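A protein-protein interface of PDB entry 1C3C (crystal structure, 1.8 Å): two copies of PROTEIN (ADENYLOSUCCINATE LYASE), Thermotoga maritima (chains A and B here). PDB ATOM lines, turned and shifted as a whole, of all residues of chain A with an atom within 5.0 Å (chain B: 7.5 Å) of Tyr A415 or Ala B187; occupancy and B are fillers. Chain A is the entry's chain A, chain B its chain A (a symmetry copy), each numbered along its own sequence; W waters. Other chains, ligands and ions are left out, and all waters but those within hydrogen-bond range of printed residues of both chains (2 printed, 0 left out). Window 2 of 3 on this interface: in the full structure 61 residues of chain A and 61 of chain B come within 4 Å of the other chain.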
ATOM      1  N   GLU A 145       8.874  -2.747 -26.773  1.00  0.00           N
ATOM      2  CA  GLU A 145      10.068  -3.031 -25.977  1.00  0.00           C
ATOM      3  C   GLU A 145      10.499  -4.462 -26.309  1.00  0.00           C
ATOM      4  O   GLU A 145       9.661  -5.260 -26.725  1.00  0.00           O
ATOM      5  CB  GLU A 145       9.801  -3.076 -24.437  1.00  0.00           C
ATOM      6  CG  GLU A 145       9.503  -1.678 -23.921  1.00  0.00           C
ATOM      7  CD  GLU A 145       9.233  -1.565 -22.450  1.00  0.00           C
ATOM      8  OE1 GLU A 145       9.055  -2.589 -21.766  1.00  0.00           O
ATOM      9  OE2 GLU A 145       9.226  -0.381 -21.994  1.00  0.00           O
ATOM     10  N   ARG A 355      13.941   4.438 -21.420  1.00  0.00           N
ATOM     11  CA  ARG A 355      15.040   4.396 -20.439  1.00  0.00           C
ATOM     12  C   ARG A 355      15.852   5.689 -20.472  1.00  0.00           C
ATOM     13  O   ARG A 355      16.264   6.152 -19.389  1.00  0.00           O
ATOM     14  CB  ARG A 355      15.952   3.201 -20.742  1.00  0.00           C
ATOM     15  CG  ARG A 355      15.166   1.881 -20.672  1.00  0.00           C
ATOM     16  CD  ARG A 355      16.125   0.756 -20.255  1.00  0.00           C
ATOM     17  NE  ARG A 355      16.560   0.937 -18.870  1.00  0.00           N
ATOM     18  CZ  ARG A 355      17.654   0.458 -18.326  1.00  0.00           C
ATOM     19  NH1 ARG A 355      17.923   0.675 -17.028  1.00  0.00           N
ATOM     20  NH2 ARG A 355      18.488  -0.268 -19.048  1.00  0.00           N
ATOM     21  N   ASP A 412      21.042  -1.983 -23.325  1.00  0.00           N
ATOM     22  CA  ASP A 412      21.193  -3.397 -23.040  1.00  0.00           C
ATOM     23  C   ASP A 412      19.878  -4.159 -23.113  1.00  0.00           C
ATOM     24  O   ASP A 412      18.930  -3.848 -22.371  1.00  0.00           O
ATOM     25  CB  ASP A 412      21.654  -3.423 -21.576  1.00  0.00           C
ATOM     26  CG  ASP A 412      22.728  -4.411 -21.276  1.00  0.00           C
ATOM     27  OD1 ASP A 412      22.712  -5.423 -21.996  1.00  0.00           O
ATOM     28  OD2 ASP A 412      23.514  -4.129 -20.331  1.00  0.00           O
ATOM     29  N   ILE A 413      19.799  -5.197 -23.923  1.00  0.00           N
ATOM     30  CA  ILE A 413      18.582  -6.033 -24.005  1.00  0.00           C
ATOM     31  C   ILE A 413      18.342  -6.818 -22.742  1.00  0.00           C
ATOM     32  O   ILE A 413      17.221  -7.212 -22.395  1.00  0.00           O
ATOM     33  CB  ILE A 413      18.674  -6.991 -25.217  1.00  0.00           C
ATOM     34  CG1 ILE A 413      18.482  -6.021 -26.404  1.00  0.00           C
ATOM     35  CG2 ILE A 413      17.598  -8.047 -25.310  1.00  0.00           C
ATOM     36  CD1 ILE A 413      18.589  -6.617 -27.794  1.00  0.00           C
ATOM     37  N   SER A 414      19.402  -7.076 -21.975  1.00  0.00           N
ATOM     38  CA  SER A 414      19.270  -7.857 -20.755  1.00  0.00           C
ATOM     39  C   SER A 414      18.341  -7.236 -19.730  1.00  0.00           C
ATOM     40  O   SER A 414      17.684  -7.968 -18.983  1.00  0.00           O
ATOM     41  CB  SER A 414      20.684  -8.131 -20.190  1.00  0.00           C
ATOM     42  OG  SER A 414      21.143  -6.986 -19.481  1.00  0.00           O
ATOM     43  N   TYR A 415      18.198  -5.908 -19.652  1.00  0.00           N
ATOM     44  CA  TYR A 415      17.172  -5.264 -18.847  1.00  0.00           C
ATOM     45  C   TYR A 415      15.779  -5.830 -19.121  1.00  0.00           C
ATOM     46  O   TYR A 415      14.986  -5.950 -18.171  1.00  0.00           O
ATOM     47  CB  TYR A 415      17.188  -3.752 -19.106  1.00  0.00           C
ATOM     48  CG  TYR A 415      16.127  -2.939 -18.415  1.00  0.00           C
ATOM     49  CD1 TYR A 415      16.300  -2.396 -17.133  1.00  0.00           C
ATOM     50  CD2 TYR A 415      14.893  -2.741 -19.073  1.00  0.00           C
ATOM     51  CE1 TYR A 415      15.264  -1.656 -16.553  1.00  0.00           C
ATOM     52  CE2 TYR A 415      13.894  -1.978 -18.509  1.00  0.00           C
ATOM     53  CZ  TYR A 415      14.085  -1.464 -17.249  1.00  0.00           C
ATOM     54  OH  TYR A 415      13.081  -0.713 -16.686  1.00  0.00           O
ATOM     55  N   TYR A 416      15.484  -6.152 -20.387  1.00  0.00           N
ATOM     56  CA  TYR A 416      14.092  -6.519 -20.752  1.00  0.00           C
ATOM     57  C   TYR A 416      13.812  -7.990 -20.500  1.00  0.00           C
ATOM     58  O   TYR A 416      12.655  -8.399 -20.404  1.00  0.00           O
ATOM     59  CB  TYR A 416      13.849  -6.145 -22.235  1.00  0.00           C
ATOM     60  CG  TYR A 416      13.835  -4.618 -22.315  1.00  0.00           C
ATOM     61  CD1 TYR A 416      14.948  -3.909 -22.691  1.00  0.00           C
ATOM     62  CD2 TYR A 416      12.662  -3.930 -21.959  1.00  0.00           C
ATOM     63  CE1 TYR A 416      14.907  -2.523 -22.719  1.00  0.00           C
ATOM     64  CE2 TYR A 416      12.604  -2.549 -21.992  1.00  0.00           C
ATOM     65  CZ  TYR A 416      13.740  -1.857 -22.382  1.00  0.00           C
ATOM     66  OH  TYR A 416      13.734  -0.470 -22.423  1.00  0.00           O
ATOM     67  N   LEU A 417      14.862  -8.821 -20.473  1.00  0.00           N
ATOM     68  CA  LEU A 417      14.678 -10.262 -20.360  1.00  0.00           C
ATOM     69  C   LEU A 417      14.927 -10.784 -18.958  1.00  0.00           C
ATOM     70  O   LEU A 417      14.892 -12.013 -18.734  1.00  0.00           O
ATOM     71  CB  LEU A 417      15.613 -11.027 -21.312  1.00  0.00           C
ATOM     72  CG  LEU A 417      15.518 -10.670 -22.795  1.00  0.00           C
ATOM     73  CD1 LEU A 417      16.112 -11.737 -23.728  1.00  0.00           C
ATOM     74  CD2 LEU A 417      14.104 -10.438 -23.232  1.00  0.00           C
ATOM     75  N   LYS A 418      15.112  -9.896 -17.982  1.00  0.00           N
ATOM     76  CA  LYS A 418      15.564 -10.350 -16.663  1.00  0.00           C
ATOM     77  C   LYS A 418      14.552 -11.201 -15.904  1.00  0.00           C
ATOM     78  O   LYS A 418      14.897 -11.828 -14.890  1.00  0.00           O
ATOM     79  CB  LYS A 418      15.913  -9.097 -15.854  1.00  0.00           C
ATOM     80  CG  LYS A 418      14.720  -8.166 -15.562  1.00  0.00           C
ATOM     81  CD  LYS A 418      15.250  -7.067 -14.628  1.00  0.00           C
ATOM     82  CE  LYS A 418      14.156  -6.009 -14.445  1.00  0.00           C
ATOM     83  NZ  LYS A 418      14.295  -4.947 -15.516  1.00  0.00           N
ATOM     84  N   GLY B  90       6.224   2.268 -13.215  1.00  0.00           N
ATOM     85  CA  GLY B  90       6.566   1.111 -14.052  1.00  0.00           C
ATOM     86  C   GLY B  90       5.383   0.471 -14.775  1.00  0.00           C
ATOM     87  O   GLY B  90       5.534  -0.470 -15.581  1.00  0.00           O
ATOM     88  N   SER B 180       2.300  -6.076 -15.125  1.00  0.00           N
ATOM     89  CA  SER B 180       3.526  -6.672 -15.724  1.00  0.00           C
ATOM     90  C   SER B 180       4.172  -5.689 -16.699  1.00  0.00           C
ATOM     91  O   SER B 180       5.204  -5.983 -17.286  1.00  0.00           O
ATOM     92  CB  SER B 180       3.194  -7.995 -16.428  1.00  0.00           C
ATOM     93  OG  SER B 180       2.204  -7.801 -17.402  1.00  0.00           O
ATOM     94  N   GLY B 181       3.559  -4.521 -16.844  1.00  0.00           N
ATOM     95  CA  GLY B 181       4.163  -3.446 -17.655  1.00  0.00           C
ATOM     96  C   GLY B 181       4.036  -3.667 -19.147  1.00  0.00           C
ATOM     97  O   GLY B 181       3.279  -4.511 -19.641  1.00  0.00           O
ATOM     98  N   ALA B 182       4.724  -2.818 -19.892  1.00  0.00           N
ATOM     99  CA  ALA B 182       4.434  -2.573 -21.312  1.00  0.00           C
ATOM    100  C   ALA B 182       4.241  -3.807 -22.176  1.00  0.00           C
ATOM    101  O   ALA B 182       3.279  -3.740 -22.977  1.00  0.00           O
ATOM    102  CB  ALA B 182       5.602  -1.790 -21.902  1.00  0.00           C
ATOM    103  N   VAL B 183       5.127  -4.810 -22.193  1.00  0.00           N
ATOM    104  CA  VAL B 183       4.885  -5.992 -23.038  1.00  0.00           C
ATOM    105  C   VAL B 183       4.766  -7.238 -22.165  1.00  0.00           C
ATOM    106  O   VAL B 183       4.873  -8.370 -22.638  1.00  0.00           O
ATOM    107  CB  VAL B 183       5.941  -6.179 -24.144  1.00  0.00           C
ATOM    108  CG1 VAL B 183       5.786  -5.021 -25.160  1.00  0.00           C
ATOM    109  CG2 VAL B 183       7.368  -6.216 -23.620  1.00  0.00           C
ATOM    110  N   GLY B 184       4.480  -7.079 -20.869  1.00  0.00           N
ATOM    111  CA  GLY B 184       4.064  -8.225 -20.032  1.00  0.00           C
ATOM    112  C   GLY B 184       5.237  -9.014 -19.446  1.00  0.00           C
ATOM    113  O   GLY B 184       5.020 -10.076 -18.879  1.00  0.00           O
ATOM    114  N   ASN B 185       6.444  -8.481 -19.543  1.00  0.00           N
ATOM    115  CA  ASN B 185       7.614  -9.263 -19.112  1.00  0.00           C
ATOM    116  C   ASN B 185       8.310  -8.675 -17.896  1.00  0.00           C
ATOM    117  O   ASN B 185       9.433  -9.116 -17.564  1.00  0.00           O
ATOM    118  CB  ASN B 185       8.618  -9.449 -20.236  1.00  0.00           C
ATOM    119  CG  ASN B 185       9.112  -8.161 -20.830  1.00  0.00           C
ATOM    120  OD1 ASN B 185       8.978  -7.074 -20.237  1.00  0.00           O
ATOM    121  ND2 ASN B 185       9.724  -8.256 -22.013  1.00  0.00           N
ATOM    122  N   TYR B 186       7.713  -7.750 -17.165  1.00  0.00           N
ATOM    123  CA  TYR B 186       8.268  -7.292 -15.870  1.00  0.00           C
ATOM    124  C   TYR B 186       9.557  -6.517 -16.064  1.00  0.00           C
ATOM    125  O   TYR B 186      10.275  -6.349 -15.056  1.00  0.00           O
ATOM    126  CB  TYR B 186       8.398  -8.373 -14.779  1.00  0.00           C
ATOM    127  CG  TYR B 186       7.108  -9.173 -14.621  1.00  0.00           C
ATOM    128  CD1 TYR B 186       7.064 -10.439 -15.245  1.00  0.00           C
ATOM    129  CD2 TYR B 186       5.993  -8.693 -13.961  1.00  0.00           C
ATOM    130  CE1 TYR B 186       5.882 -11.190 -15.194  1.00  0.00           C
ATOM    131  CE2 TYR B 186       4.828  -9.448 -13.875  1.00  0.00           C
ATOM    132  CZ  TYR B 186       4.797 -10.683 -14.525  1.00  0.00           C
ATOM    133  OH  TYR B 186       3.685 -11.452 -14.482  1.00  0.00           O
ATOM    134  N   ALA B 187       9.802  -5.945 -17.252  1.00  0.00           N
ATOM    135  CA  ALA B 187      11.042  -5.170 -17.423  1.00  0.00           C
ATOM    136  C   ALA B 187      10.972  -3.932 -16.511  1.00  0.00           C
ATOM    137  O   ALA B 187      11.996  -3.513 -15.957  1.00  0.00           O
ATOM    138  CB  ALA B 187      11.140  -4.699 -18.874  1.00  0.00           C
ATOM    139  N   ASN B 188       9.772  -3.385 -16.316  1.00  0.00           N
ATOM    140  CA  ASN B 188       9.609  -2.112 -15.620  1.00  0.00           C
ATOM    141  C   ASN B 188       8.872  -2.214 -14.295  1.00  0.00           C
ATOM    142  O   ASN B 188       8.855  -1.199 -13.566  1.00  0.00           O
ATOM    143  CB  ASN B 188       8.866  -1.080 -16.496  1.00  0.00           C
ATOM    144  CG  ASN B 188       9.464  -1.019 -17.907  1.00  0.00           C
ATOM    145  OD1 ASN B 188      10.678  -0.867 -18.074  1.00  0.00           O
ATOM    146  ND2 ASN B 188       8.609  -1.154 -18.905  1.00  0.00           N
ATOM    147  N   VAL B 189       8.284  -3.341 -13.945  1.00  0.00           N
ATOM    148  CA  VAL B 189       7.627  -3.475 -12.627  1.00  0.00           C
ATOM    149  C   VAL B 189       7.866  -4.928 -12.217  1.00  0.00           C
ATOM    150  O   VAL B 189       7.696  -5.773 -13.078  1.00  0.00           O
ATOM    151  CB  VAL B 189       6.141  -3.108 -12.714  1.00  0.00           C
ATOM    152  CG1 VAL B 189       5.394  -3.817 -13.848  1.00  0.00           C
ATOM    153  CG2 VAL B 189       5.449  -3.466 -11.380  1.00  0.00           C
ATOM    154  N   PRO B 190       8.246  -5.245 -10.978  1.00  0.00           N
ATOM    155  CA  PRO B 190       8.710  -6.610 -10.681  1.00  0.00           C
ATOM    156  C   PRO B 190       7.544  -7.573 -10.518  1.00  0.00           C
ATOM    157  O   PRO B 190       6.481  -7.173 -10.038  1.00  0.00           O
ATOM    158  CB  PRO B 190       9.451  -6.496  -9.338  1.00  0.00           C
ATOM    159  CG  PRO B 190       9.597  -5.043  -9.071  1.00  0.00           C
ATOM    160  CD  PRO B 190       8.668  -4.251  -9.966  1.00  0.00           C
ATOM    161  N   PRO B 191       7.745  -8.861 -10.776  1.00  0.00           N
ATOM    162  CA  PRO B 191       6.706  -9.860 -10.609  1.00  0.00           C
ATOM    163  C   PRO B 191       6.300 -10.029  -9.162  1.00  0.00           C
ATOM    164  O   PRO B 191       5.148 -10.316  -8.859  1.00  0.00           O
ATOM    165  CB  PRO B 191       7.264 -11.134 -11.228  1.00  0.00           C
ATOM    166  CG  PRO B 191       8.754 -10.940 -11.146  1.00  0.00           C
ATOM    167  CD  PRO B 191       9.012  -9.455 -11.291  1.00  0.00           C
HETATM  168  O   HOH W   1       7.721  -4.643 -20.619  1.00  0.00           O
HETATM  169  O   HOH W   2      12.530  -0.737 -14.112  1.00  0.00           O
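OE1 of Glu A145 is in hydrogen-bond range of ND2 of Asn B188.
The side-chain hydroxyl (OH) of Tyr A415 sits at hydrogen-bond distance from the backbone carbonyl oxygen (O) of Ala B187.
OH of Tyr A415 sits at hydrogen-bond distance from OD1 of Asn B188, 2.8 Å away.
The side-chain amide nitrogen of Asn B185 sits at hydrogen-bond distance from the backbone carbonyl oxygen of Tyr A416 (3.3 Å).
O of Ala B187 is in hydrogen-bond range of NZ of Lys A418, at 2.7 Å.
The backbone carbonyl oxygen of Tyr A415 lies within hydrogen-bond range of the side-chain amino group of Lys A418, 2.9 Å away.
N of Tyr B186 is in hydrogen-bond range of O of Ser B180.
N of Ala B187 sits close to OD1 of Asn B185, 3.3 Å away.
Glu A145 touches Ala B182 (OE1 to CB, 3.5 Å).
O of Glu A145 touches CG2 of Val B183 (3.98 Å).
CB of Ala B187 touches CD2 of Tyr A416 (3.5 Å).
O of Tyr B186 touches CE of Lys A418 (3.9 Å).
Printed residues of chain B within 4 Å of Tyr A415: Ala B187 and Asn B188.
Ala B187 touches three residues of chain A.
Ser A414 touches none of the printed residues of chain B.
Printed residues of chain A within 4 Å of Val B183: Glu A145.
Printed residues of chain B within 4 Å of Lys A418: Tyr B186 and Ala B187.
Printed residues of chain B within 4 Å of Tyr A416: Asn B185 (3.3 Å) and Ala B187 (3.5 Å).
Printed residues of chain A within 4 Å of Asn B185: Tyr A416.
Of the printed residues of chain A, Asn B188 touches Glu A145 (3.2 Å) and Tyr A415 (2.8 Å).
Gly B90 touches none of the printed residues of chain A.
Ile A413 touches none of the printed residues of chain B.
The nearest residue of chain B that does not touch Tyr A415 is Tyr B186 (5.7 Å).
The nearest printed residue of chain A that does not touch Tyr B186 is Tyr A416 (5.7 Å).
Of the 9 printed residues of chain A, 4 touch a printed residue of chain B.
Among the printed residues, 9 pairs touch across the chains.
No position is printed for both chains.
Water W2 lies within hydrogen-bond range of the side-chain hydroxyl of Tyr A415 (2.6 Å) and the backbone carbonyl oxygen of Ala B187 (3.4 Å).
Water W1 lies within hydrogen-bond range of OE1 of Glu A145 (2.7 Å), OD1 of Asn B185 (2.8 Å) and N of Val B183 (3.0 Å).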
